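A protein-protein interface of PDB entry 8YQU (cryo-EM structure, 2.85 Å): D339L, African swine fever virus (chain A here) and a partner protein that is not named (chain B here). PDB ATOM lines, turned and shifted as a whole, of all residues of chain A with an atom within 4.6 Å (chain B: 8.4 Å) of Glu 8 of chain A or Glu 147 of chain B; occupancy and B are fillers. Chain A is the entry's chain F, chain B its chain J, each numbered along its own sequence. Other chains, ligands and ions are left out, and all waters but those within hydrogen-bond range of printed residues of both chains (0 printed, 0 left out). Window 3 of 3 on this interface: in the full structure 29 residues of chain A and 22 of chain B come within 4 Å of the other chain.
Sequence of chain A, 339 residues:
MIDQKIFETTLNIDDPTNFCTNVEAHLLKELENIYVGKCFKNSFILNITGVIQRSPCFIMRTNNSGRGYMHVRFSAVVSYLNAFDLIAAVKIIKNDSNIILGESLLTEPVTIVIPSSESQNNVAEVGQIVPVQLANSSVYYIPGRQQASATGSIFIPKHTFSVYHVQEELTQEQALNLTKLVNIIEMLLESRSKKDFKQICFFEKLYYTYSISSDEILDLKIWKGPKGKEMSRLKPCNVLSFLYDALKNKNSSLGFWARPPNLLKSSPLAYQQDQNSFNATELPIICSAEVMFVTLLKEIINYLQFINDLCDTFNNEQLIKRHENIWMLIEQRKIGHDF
Printed residues of chain A that touch a printed residue of chain B: Ile 6, Glu 8, Lys 41 and Arg 73.
Among the printed residues, 6 pairs touch across the chains.
Among the printed residues, no Asp or Glu carboxylate lies within 4 Å of a Lys or Arg side-chain nitrogen of the other chain.
Glu 8 of chain A touches just one residue of chain B: Glu 147.
Printed residues of chain B within 4 Å of Lys 41 of chain A: Ile 148 (3.3 Å), Gly 149 (3.7 Å) and Ser 150 (3.6 Å).
Of the printed residues of chain B, Arg 73 of chain A touches Leu 231.
Of chain A, only Glu 8 comes within 4 Å of Glu 147 of chain B.
Of the printed residues of chain A, Ile 148 of chain B touches Lys 41.
Printed residues of chain A within 4 Å of Ser 150 of chain B: Lys 41 (3.6 Å).
Printed residues of chain A within 4 Å of Val 227 of chain B: Ile 6 (3.7 Å).
The nearest printed residue of chain A that does not touch Glu 147 of chain B is Lys 41 of chain A (4.7 Å).
The nearest printed residue of chain A that does not touch Val 227 of chain B is Arg 73 of chain A (5.7 Å).
The side-chain amino group of Lys 41 of chain A lies within hydrogen-bond range of the backbone carbonyl oxygen of Ile 148 of chain B (3.3 Å).
CD1 of Ile 6 of chain A touches CG1 of Val 227 of chain B, at 3.7 Å.
Glu 8 of chain A touches Glu 147 of chain B.
Lys 41 of chain A touches Gly 149 of chain B (CB to O, 3.7 Å).
CG of Lys 41 of chain A touches CB of Ser 150 of chain B, 3.6 Å away.
Arg 73 of chain A touches Leu 231 of chain B (NH1 to CD2, 3.2 Å).
The side-chain carboxylate (OE2) of Glu 147 of chain B lies within salt-bridge range of the side-chain amino group (NZ) of Lys 230 of chain B, 3.0 Å away.
The side-chain amino group (NZ) of Lys 41 of chain A sits at hydrogen-bond distance from the backbone carbonyl oxygen (O) of Glu 8 of chain A, at 3.3 Å.
The guanidinium group (NH2) of Arg 73 of chain A lies within salt-bridge range of the side-chain carboxylate (OE2) of Glu 8 of chain A.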
ATOM      1  N   ILE A   6     -26.103   4.969 -22.043  1.00  0.00           N
ATOM      2  CA  ILE A   6     -25.099   5.703 -21.280  1.00  0.00           C
ATOM      3  C   ILE A   6     -24.320   6.594 -22.237  1.00  0.00           C
ATOM      4  O   ILE A   6     -23.875   6.135 -23.295  1.00  0.00           O
ATOM      5  CB  ILE A   6     -24.155   4.751 -20.523  1.00  0.00           C
ATOM      6  CG1 ILE A   6     -24.942   3.917 -19.512  1.00  0.00           C
ATOM      7  CG2 ILE A   6     -23.056   5.532 -19.822  1.00  0.00           C
ATOM      8  CD1 ILE A   6     -24.129   2.828 -18.855  1.00  0.00           C
ATOM      9  N   PHE A   7     -24.156   7.864 -21.866  1.00  0.00           N
ATOM     10  CA  PHE A   7     -23.464   8.844 -22.687  1.00  0.00           C
ATOM     11  C   PHE A   7     -22.339   9.495 -21.894  1.00  0.00           C
ATOM     12  O   PHE A   7     -22.368   9.541 -20.659  1.00  0.00           O
ATOM     13  CB  PHE A   7     -24.413   9.939 -23.184  1.00  0.00           C
ATOM     14  CG  PHE A   7     -25.532   9.437 -24.044  1.00  0.00           C
ATOM     15  CD1 PHE A   7     -26.712   8.992 -23.478  1.00  0.00           C
ATOM     16  CD2 PHE A   7     -25.413   9.430 -25.423  1.00  0.00           C
ATOM     17  CE1 PHE A   7     -27.745   8.538 -24.267  1.00  0.00           C
ATOM     18  CE2 PHE A   7     -26.445   8.977 -26.218  1.00  0.00           C
ATOM     19  CZ  PHE A   7     -27.612   8.531 -25.639  1.00  0.00           C
ATOM     20  N   GLU A   8     -21.353  10.008 -22.625  1.00  0.00           N
ATOM     21  CA  GLU A   8     -20.257  10.787 -22.069  1.00  0.00           C
ATOM     22  C   GLU A   8     -20.224  12.143 -22.756  1.00  0.00           C
ATOM     23  O   GLU A   8     -20.398  12.233 -23.975  1.00  0.00           O
ATOM     24  CB  GLU A   8     -18.916  10.078 -22.259  1.00  0.00           C
ATOM     25  CG  GLU A   8     -18.806   8.746 -21.546  1.00  0.00           C
ATOM     26  CD  GLU A   8     -17.418   8.152 -21.650  1.00  0.00           C
ATOM     27  OE1 GLU A   8     -16.567   8.748 -22.343  1.00  0.00           O
ATOM     28  OE2 GLU A   8     -17.179   7.088 -21.046  1.00  0.00           O
ATOM     29  N   THR A   9     -19.999  13.199 -21.977  1.00  0.00           N
ATOM     30  CA  THR A   9     -20.001  14.544 -22.530  1.00  0.00           C
ATOM     31  C   THR A   9     -19.162  15.455 -21.646  1.00  0.00           C
ATOM     32  O   THR A   9     -18.700  15.064 -20.572  1.00  0.00           O
ATOM     33  CB  THR A   9     -21.424  15.094 -22.662  1.00  0.00           C
ATOM     34  OG1 THR A   9     -21.398  16.316 -23.410  1.00  0.00           O
ATOM     35  CG2 THR A   9     -22.019  15.361 -21.290  1.00  0.00           C
ATOM     36  N   LYS A  41     -25.597  11.033 -30.865  1.00  0.00           N
ATOM     37  CA  LYS A  41     -24.900   9.748 -30.827  1.00  0.00           C
ATOM     38  C   LYS A  41     -25.826   8.600 -31.237  1.00  0.00           C
ATOM     39  O   LYS A  41     -26.003   7.616 -30.516  1.00  0.00           O
ATOM     40  CB  LYS A  41     -24.281   9.502 -29.447  1.00  0.00           C
ATOM     41  CG  LYS A  41     -23.000  10.281 -29.210  1.00  0.00           C
ATOM     42  CD  LYS A  41     -22.306   9.842 -27.937  1.00  0.00           C
ATOM     43  CE  LYS A  41     -20.984  10.569 -27.760  1.00  0.00           C
ATOM     44  NZ  LYS A  41     -20.280  10.143 -26.521  1.00  0.00           N
ATOM     45  N   VAL A  72     -18.981  14.640 -17.736  1.00  0.00           N
ATOM     46  CA  VAL A  72     -20.169  14.008 -17.176  1.00  0.00           C
ATOM     47  C   VAL A  72     -20.447  12.717 -17.931  1.00  0.00           C
ATOM     48  O   VAL A  72     -20.555  12.720 -19.163  1.00  0.00           O
ATOM     49  CB  VAL A  72     -21.392  14.941 -17.237  1.00  0.00           C
ATOM     50  CG1 VAL A  72     -22.552  14.334 -16.471  1.00  0.00           C
ATOM     51  CG2 VAL A  72     -21.040  16.312 -16.693  1.00  0.00           C
ATOM     52  N   ARG A  73     -20.575  11.622 -17.189  1.00  0.00           N
ATOM     53  CA  ARG A  73     -21.009  10.335 -17.718  1.00  0.00           C
ATOM     54  C   ARG A  73     -22.387  10.053 -17.134  1.00  0.00           C
ATOM     55  O   ARG A  73     -22.522   9.823 -15.926  1.00  0.00           O
ATOM     56  CB  ARG A  73     -20.004   9.239 -17.367  1.00  0.00           C
ATOM     57  CG  ARG A  73     -20.335   7.861 -17.907  1.00  0.00           C
ATOM     58  CD  ARG A  73     -19.215   6.884 -17.579  1.00  0.00           C
ATOM     59  NE  ARG A  73     -18.006   7.186 -18.336  1.00  0.00           N
ATOM     60  CZ  ARG A  73     -16.822   6.629 -18.122  1.00  0.00           C
ATOM     61  NH1 ARG A  73     -16.627   5.774 -17.134  1.00  0.00           N
ATOM     62  NH2 ARG A  73     -15.806   6.940 -18.921  1.00  0.00           N
ATOM     63  N   GLN B 140     -12.084  -5.794 -25.435  1.00  0.00           N
ATOM     64  CA  GLN B 140     -11.663  -4.419 -25.194  1.00  0.00           C
ATOM     65  C   GLN B 140     -12.091  -3.493 -26.325  1.00  0.00           C
ATOM     66  O   GLN B 140     -12.442  -2.337 -26.076  1.00  0.00           O
ATOM     67  CB  GLN B 140     -10.148  -4.361 -25.002  1.00  0.00           C
ATOM     68  CG  GLN B 140      -9.653  -5.124 -23.783  1.00  0.00           C
ATOM     69  CD  GLN B 140     -10.136  -4.518 -22.480  1.00  0.00           C
ATOM     70  OE1 GLN B 140     -10.201  -3.298 -22.335  1.00  0.00           O
ATOM     71  NE2 GLN B 140     -10.477  -5.372 -21.521  1.00  0.00           N
ATOM     72  N   CYS B 141     -12.068  -3.977 -27.569  1.00  0.00           N
ATOM     73  CA  CYS B 141     -12.538  -3.165 -28.690  1.00  0.00           C
ATOM     74  C   CYS B 141     -14.020  -2.841 -28.552  1.00  0.00           C
ATOM     75  O   CYS B 141     -14.449  -1.703 -28.793  1.00  0.00           O
ATOM     76  CB  CYS B 141     -12.270  -3.891 -30.008  1.00  0.00           C
ATOM     77  SG  CYS B 141     -13.132  -3.181 -31.426  1.00  0.00           S
ATOM     78  N   PHE B 142     -14.824  -3.836 -28.172  1.00  0.00           N
ATOM     79  CA  PHE B 142     -16.251  -3.601 -27.992  1.00  0.00           C
ATOM     80  C   PHE B 142     -16.503  -2.643 -26.836  1.00  0.00           C
ATOM     81  O   PHE B 142     -17.382  -1.777 -26.918  1.00  0.00           O
ATOM     82  CB  PHE B 142     -16.974  -4.928 -27.771  1.00  0.00           C
ATOM     83  CG  PHE B 142     -18.467  -4.806 -27.743  1.00  0.00           C
ATOM     84  CD1 PHE B 142     -19.169  -4.508 -28.898  1.00  0.00           C
ATOM     85  CD2 PHE B 142     -19.172  -4.995 -26.568  1.00  0.00           C
ATOM     86  CE1 PHE B 142     -20.544  -4.396 -28.879  1.00  0.00           C
ATOM     87  CE2 PHE B 142     -20.546  -4.884 -26.543  1.00  0.00           C
ATOM     88  CZ  PHE B 142     -21.232  -4.585 -27.700  1.00  0.00           C
ATOM     89  N   MET B 143     -15.731  -2.775 -25.753  1.00  0.00           N
ATOM     90  CA  MET B 143     -15.840  -1.832 -24.645  1.00  0.00           C
ATOM     91  C   MET B 143     -15.464  -0.421 -25.077  1.00  0.00           C
ATOM     92  O   MET B 143     -16.089   0.552 -24.647  1.00  0.00           O
ATOM     93  CB  MET B 143     -14.971  -2.288 -23.475  1.00  0.00           C
ATOM     94  CG  MET B 143     -15.450  -3.569 -22.815  1.00  0.00           C
ATOM     95  SD  MET B 143     -17.091  -3.370 -22.091  1.00  0.00           S
ATOM     96  CE  MET B 143     -18.117  -4.170 -23.320  1.00  0.00           C
ATOM     97  N   ARG B 144     -14.441  -0.289 -25.922  1.00  0.00           N
ATOM     98  CA  ARG B 144     -14.048   1.031 -26.403  1.00  0.00           C
ATOM     99  C   ARG B 144     -15.137   1.652 -27.271  1.00  0.00           C
ATOM    100  O   ARG B 144     -15.422   2.851 -27.155  1.00  0.00           O
ATOM    101  CB  ARG B 144     -12.731   0.935 -27.168  1.00  0.00           C
ATOM    102  CG  ARG B 144     -12.080   2.273 -27.459  1.00  0.00           C
ATOM    103  CD  ARG B 144     -10.731   2.083 -28.127  1.00  0.00           C
ATOM    104  NE  ARG B 144     -10.047   3.349 -28.358  1.00  0.00           N
ATOM    105  CZ  ARG B 144      -8.868   3.463 -28.953  1.00  0.00           C
ATOM    106  NH1 ARG B 144      -8.209   2.402 -29.390  1.00  0.00           N
ATOM    107  NH2 ARG B 144      -8.338   4.672 -29.116  1.00  0.00           N
ATOM    108  N   MET B 145     -15.758   0.857 -28.148  1.00  0.00           N
ATOM    109  CA  MET B 145     -16.850   1.396 -28.957  1.00  0.00           C
ATOM    110  C   MET B 145     -18.042   1.781 -28.090  1.00  0.00           C
ATOM    111  O   MET B 145     -18.687   2.810 -28.330  1.00  0.00           O
ATOM    112  CB  MET B 145     -17.291   0.400 -30.023  1.00  0.00           C
ATOM    113  CG  MET B 145     -16.265   0.112 -31.087  1.00  0.00           C
ATOM    114  SD  MET B 145     -17.003  -0.978 -32.306  1.00  0.00           S
ATOM    115  CE  MET B 145     -17.068  -2.472 -31.339  1.00  0.00           C
ATOM    116  N   ALA B 146     -18.365   0.959 -27.089  1.00  0.00           N
ATOM    117  CA  ALA B 146     -19.452   1.302 -26.181  1.00  0.00           C
ATOM    118  C   ALA B 146     -19.130   2.556 -25.378  1.00  0.00           C
ATOM    119  O   ALA B 146     -20.033   3.336 -25.056  1.00  0.00           O
ATOM    120  CB  ALA B 146     -19.747   0.127 -25.252  1.00  0.00           C
ATOM    121  N   GLU B 147     -17.853   2.759 -25.044  1.00  0.00           N
ATOM    122  CA  GLU B 147     -17.427   4.016 -24.440  1.00  0.00           C
ATOM    123  C   GLU B 147     -17.668   5.179 -25.390  1.00  0.00           C
ATOM    124  O   GLU B 147     -18.130   6.247 -24.973  1.00  0.00           O
ATOM    125  CB  GLU B 147     -15.950   3.949 -24.047  1.00  0.00           C
ATOM    126  CG  GLU B 147     -15.650   2.975 -22.918  1.00  0.00           C
ATOM    127  CD  GLU B 147     -14.169   2.885 -22.607  1.00  0.00           C
ATOM    128  OE1 GLU B 147     -13.362   3.432 -23.387  1.00  0.00           O
ATOM    129  OE2 GLU B 147     -13.811   2.267 -21.582  1.00  0.00           O
ATOM    130  N   ILE B 148     -17.352   4.992 -26.673  1.00  0.00           N
ATOM    131  CA  ILE B 148     -17.758   5.970 -27.680  1.00  0.00           C
ATOM    132  C   ILE B 148     -19.278   6.038 -27.757  1.00  0.00           C
ATOM    133  O   ILE B 148     -19.867   7.125 -27.778  1.00  0.00           O
ATOM    134  CB  ILE B 148     -17.134   5.626 -29.045  1.00  0.00           C
ATOM    135  CG1 ILE B 148     -15.608   5.694 -28.970  1.00  0.00           C
ATOM    136  CG2 ILE B 148     -17.658   6.560 -30.122  1.00  0.00           C
ATOM    137  CD1 ILE B 148     -14.917   5.242 -30.238  1.00  0.00           C
ATOM    138  N   GLY B 149     -19.932   4.879 -27.796  1.00  0.00           N
ATOM    139  CA  GLY B 149     -21.377   4.807 -27.678  1.00  0.00           C
ATOM    140  C   GLY B 149     -22.158   5.512 -28.763  1.00  0.00           C
ATOM    141  O   GLY B 149     -23.235   6.051 -28.488  1.00  0.00           O
ATOM    142  N   SER B 150     -21.649   5.523 -29.996  1.00  0.00           N
ATOM    143  CA  SER B 150     -22.362   6.152 -31.100  1.00  0.00           C
ATOM    144  C   SER B 150     -22.251   5.331 -32.378  1.00  0.00           C
ATOM    145  O   SER B 150     -22.263   5.888 -33.480  1.00  0.00           O
ATOM    146  CB  SER B 150     -21.850   7.570 -31.347  1.00  0.00           C
ATOM    147  OG  SER B 150     -20.442   7.586 -31.485  1.00  0.00           O
ATOM    148  N   PHE B 151     -22.144   4.013 -32.252  1.00  0.00           N
ATOM    149  CA  PHE B 151     -21.973   3.131 -33.395  1.00  0.00           C
ATOM    150  C   PHE B 151     -23.291   2.468 -33.770  1.00  0.00           C
ATOM    151  O   PHE B 151     -24.155   2.231 -32.921  1.00  0.00           O
ATOM    152  CB  PHE B 151     -20.919   2.060 -33.104  1.00  0.00           C
ATOM    153  CG  PHE B 151     -19.509   2.569 -33.161  1.00  0.00           C
ATOM    154  CD1 PHE B 151     -18.850   2.683 -34.373  1.00  0.00           C
ATOM    155  CD2 PHE B 151     -18.845   2.939 -32.005  1.00  0.00           C
ATOM    156  CE1 PHE B 151     -17.554   3.153 -34.431  1.00  0.00           C
ATOM    157  CE2 PHE B 151     -17.548   3.410 -32.057  1.00  0.00           C
ATOM    158  CZ  PHE B 151     -16.902   3.517 -33.272  1.00  0.00           C
ATOM    159  N   LEU B 156     -21.530  -2.946 -34.110  1.00  0.00           N
ATOM    160  CA  LEU B 156     -21.377  -3.472 -32.759  1.00  0.00           C
ATOM    161  C   LEU B 156     -21.591  -4.978 -32.733  1.00  0.00           C
ATOM    162  O   LEU B 156     -20.827  -5.708 -32.094  1.00  0.00           O
ATOM    163  CB  LEU B 156     -22.353  -2.777 -31.810  1.00  0.00           C
ATOM    164  CG  LEU B 156     -22.043  -1.341 -31.387  1.00  0.00           C
ATOM    165  CD1 LEU B 156     -23.214  -0.761 -30.611  1.00  0.00           C
ATOM    166  CD2 LEU B 156     -20.768  -1.278 -30.563  1.00  0.00           C
ATOM    167  N   ALA B 223     -24.426  -4.004 -24.474  1.00  0.00           N
ATOM    168  CA  ALA B 223     -23.375  -3.000 -24.362  1.00  0.00           C
ATOM    169  C   ALA B 223     -23.623  -2.079 -23.176  1.00  0.00           C
ATOM    170  O   ALA B 223     -22.699  -1.786 -22.405  1.00  0.00           O
ATOM    171  CB  ALA B 223     -23.271  -2.198 -25.657  1.00  0.00           C
ATOM    172  N   VAL B 227     -21.157  -1.859 -19.904  1.00  0.00           N
ATOM    173  CA  VAL B 227     -20.617  -0.571 -19.470  1.00  0.00           C
ATOM    174  C   VAL B 227     -21.017  -0.285 -18.029  1.00  0.00           C
ATOM    175  O   VAL B 227     -20.197   0.165 -17.218  1.00  0.00           O
ATOM    176  CB  VAL B 227     -21.071   0.554 -20.418  1.00  0.00           C
ATOM    177  CG1 VAL B 227     -20.676   1.909 -19.858  1.00  0.00           C
ATOM    178  CG2 VAL B 227     -20.459   0.362 -21.785  1.00  0.00           C
ATOM    179  N   LYS B 230     -18.961  -2.413 -15.729  1.00  0.00           N
ATOM    180  CA  LYS B 230     -17.619  -1.849 -15.590  1.00  0.00           C
ATOM    181  C   LYS B 230     -17.619  -0.660 -14.633  1.00  0.00           C
ATOM    182  O   LYS B 230     -16.732  -0.526 -13.777  1.00  0.00           O
ATOM    183  CB  LYS B 230     -17.089  -1.438 -16.963  1.00  0.00           C
ATOM    184  CG  LYS B 230     -15.642  -0.973 -16.976  1.00  0.00           C
ATOM    185  CD  LYS B 230     -15.191  -0.656 -18.393  1.00  0.00           C
ATOM    186  CE  LYS B 230     -13.700  -0.369 -18.457  1.00  0.00           C
ATOM    187  NZ  LYS B 230     -13.243  -0.138 -19.856  1.00  0.00           N
ATOM    188  N   LEU B 231     -18.607   0.227 -14.778  1.00  0.00           N
ATOM    189  CA  LEU B 231     -18.718   1.354 -13.860  1.00  0.00           C
ATOM    190  C   LEU B 231     -18.917   0.880 -12.430  1.00  0.00           C
ATOM    191  O   LEU B 231     -18.451   1.530 -11.492  1.00  0.00           O
ATOM    192  CB  LEU B 231     -19.861   2.278 -14.282  1.00  0.00           C
ATOM    193  CG  LEU B 231     -19.749   2.838 -15.699  1.00  0.00           C
ATOM    194  CD1 LEU B 231     -20.839   3.858 -15.985  1.00  0.00           C
ATOM    195  CD2 LEU B 231     -18.375   3.436 -15.912  1.00  0.00           C
ATOM    196  N   GLU B 234     -15.236  -0.369 -11.147  1.00  0.00           N
ATOM    197  CA  GLU B 234     -14.436   0.722 -10.591  1.00  0.00           C
ATOM    198  C   GLU B 234     -15.202   1.611  -9.616  1.00  0.00           C
ATOM    199  O   GLU B 234     -14.599   2.514  -9.029  1.00  0.00           O
ATOM    200  CB  GLU B 234     -13.797   1.594 -11.683  1.00  0.00           C
ATOM    201  CG  GLU B 234     -12.650   0.941 -12.468  1.00  0.00           C
ATOM    202  CD  GLU B 234     -13.084   0.100 -13.643  1.00  0.00           C
ATOM    203  OE1 GLU B 234     -14.288   0.060 -13.937  1.00  0.00           O
ATOM    204  OE2 GLU B 234     -12.211  -0.523 -14.282  1.00  0.00           O
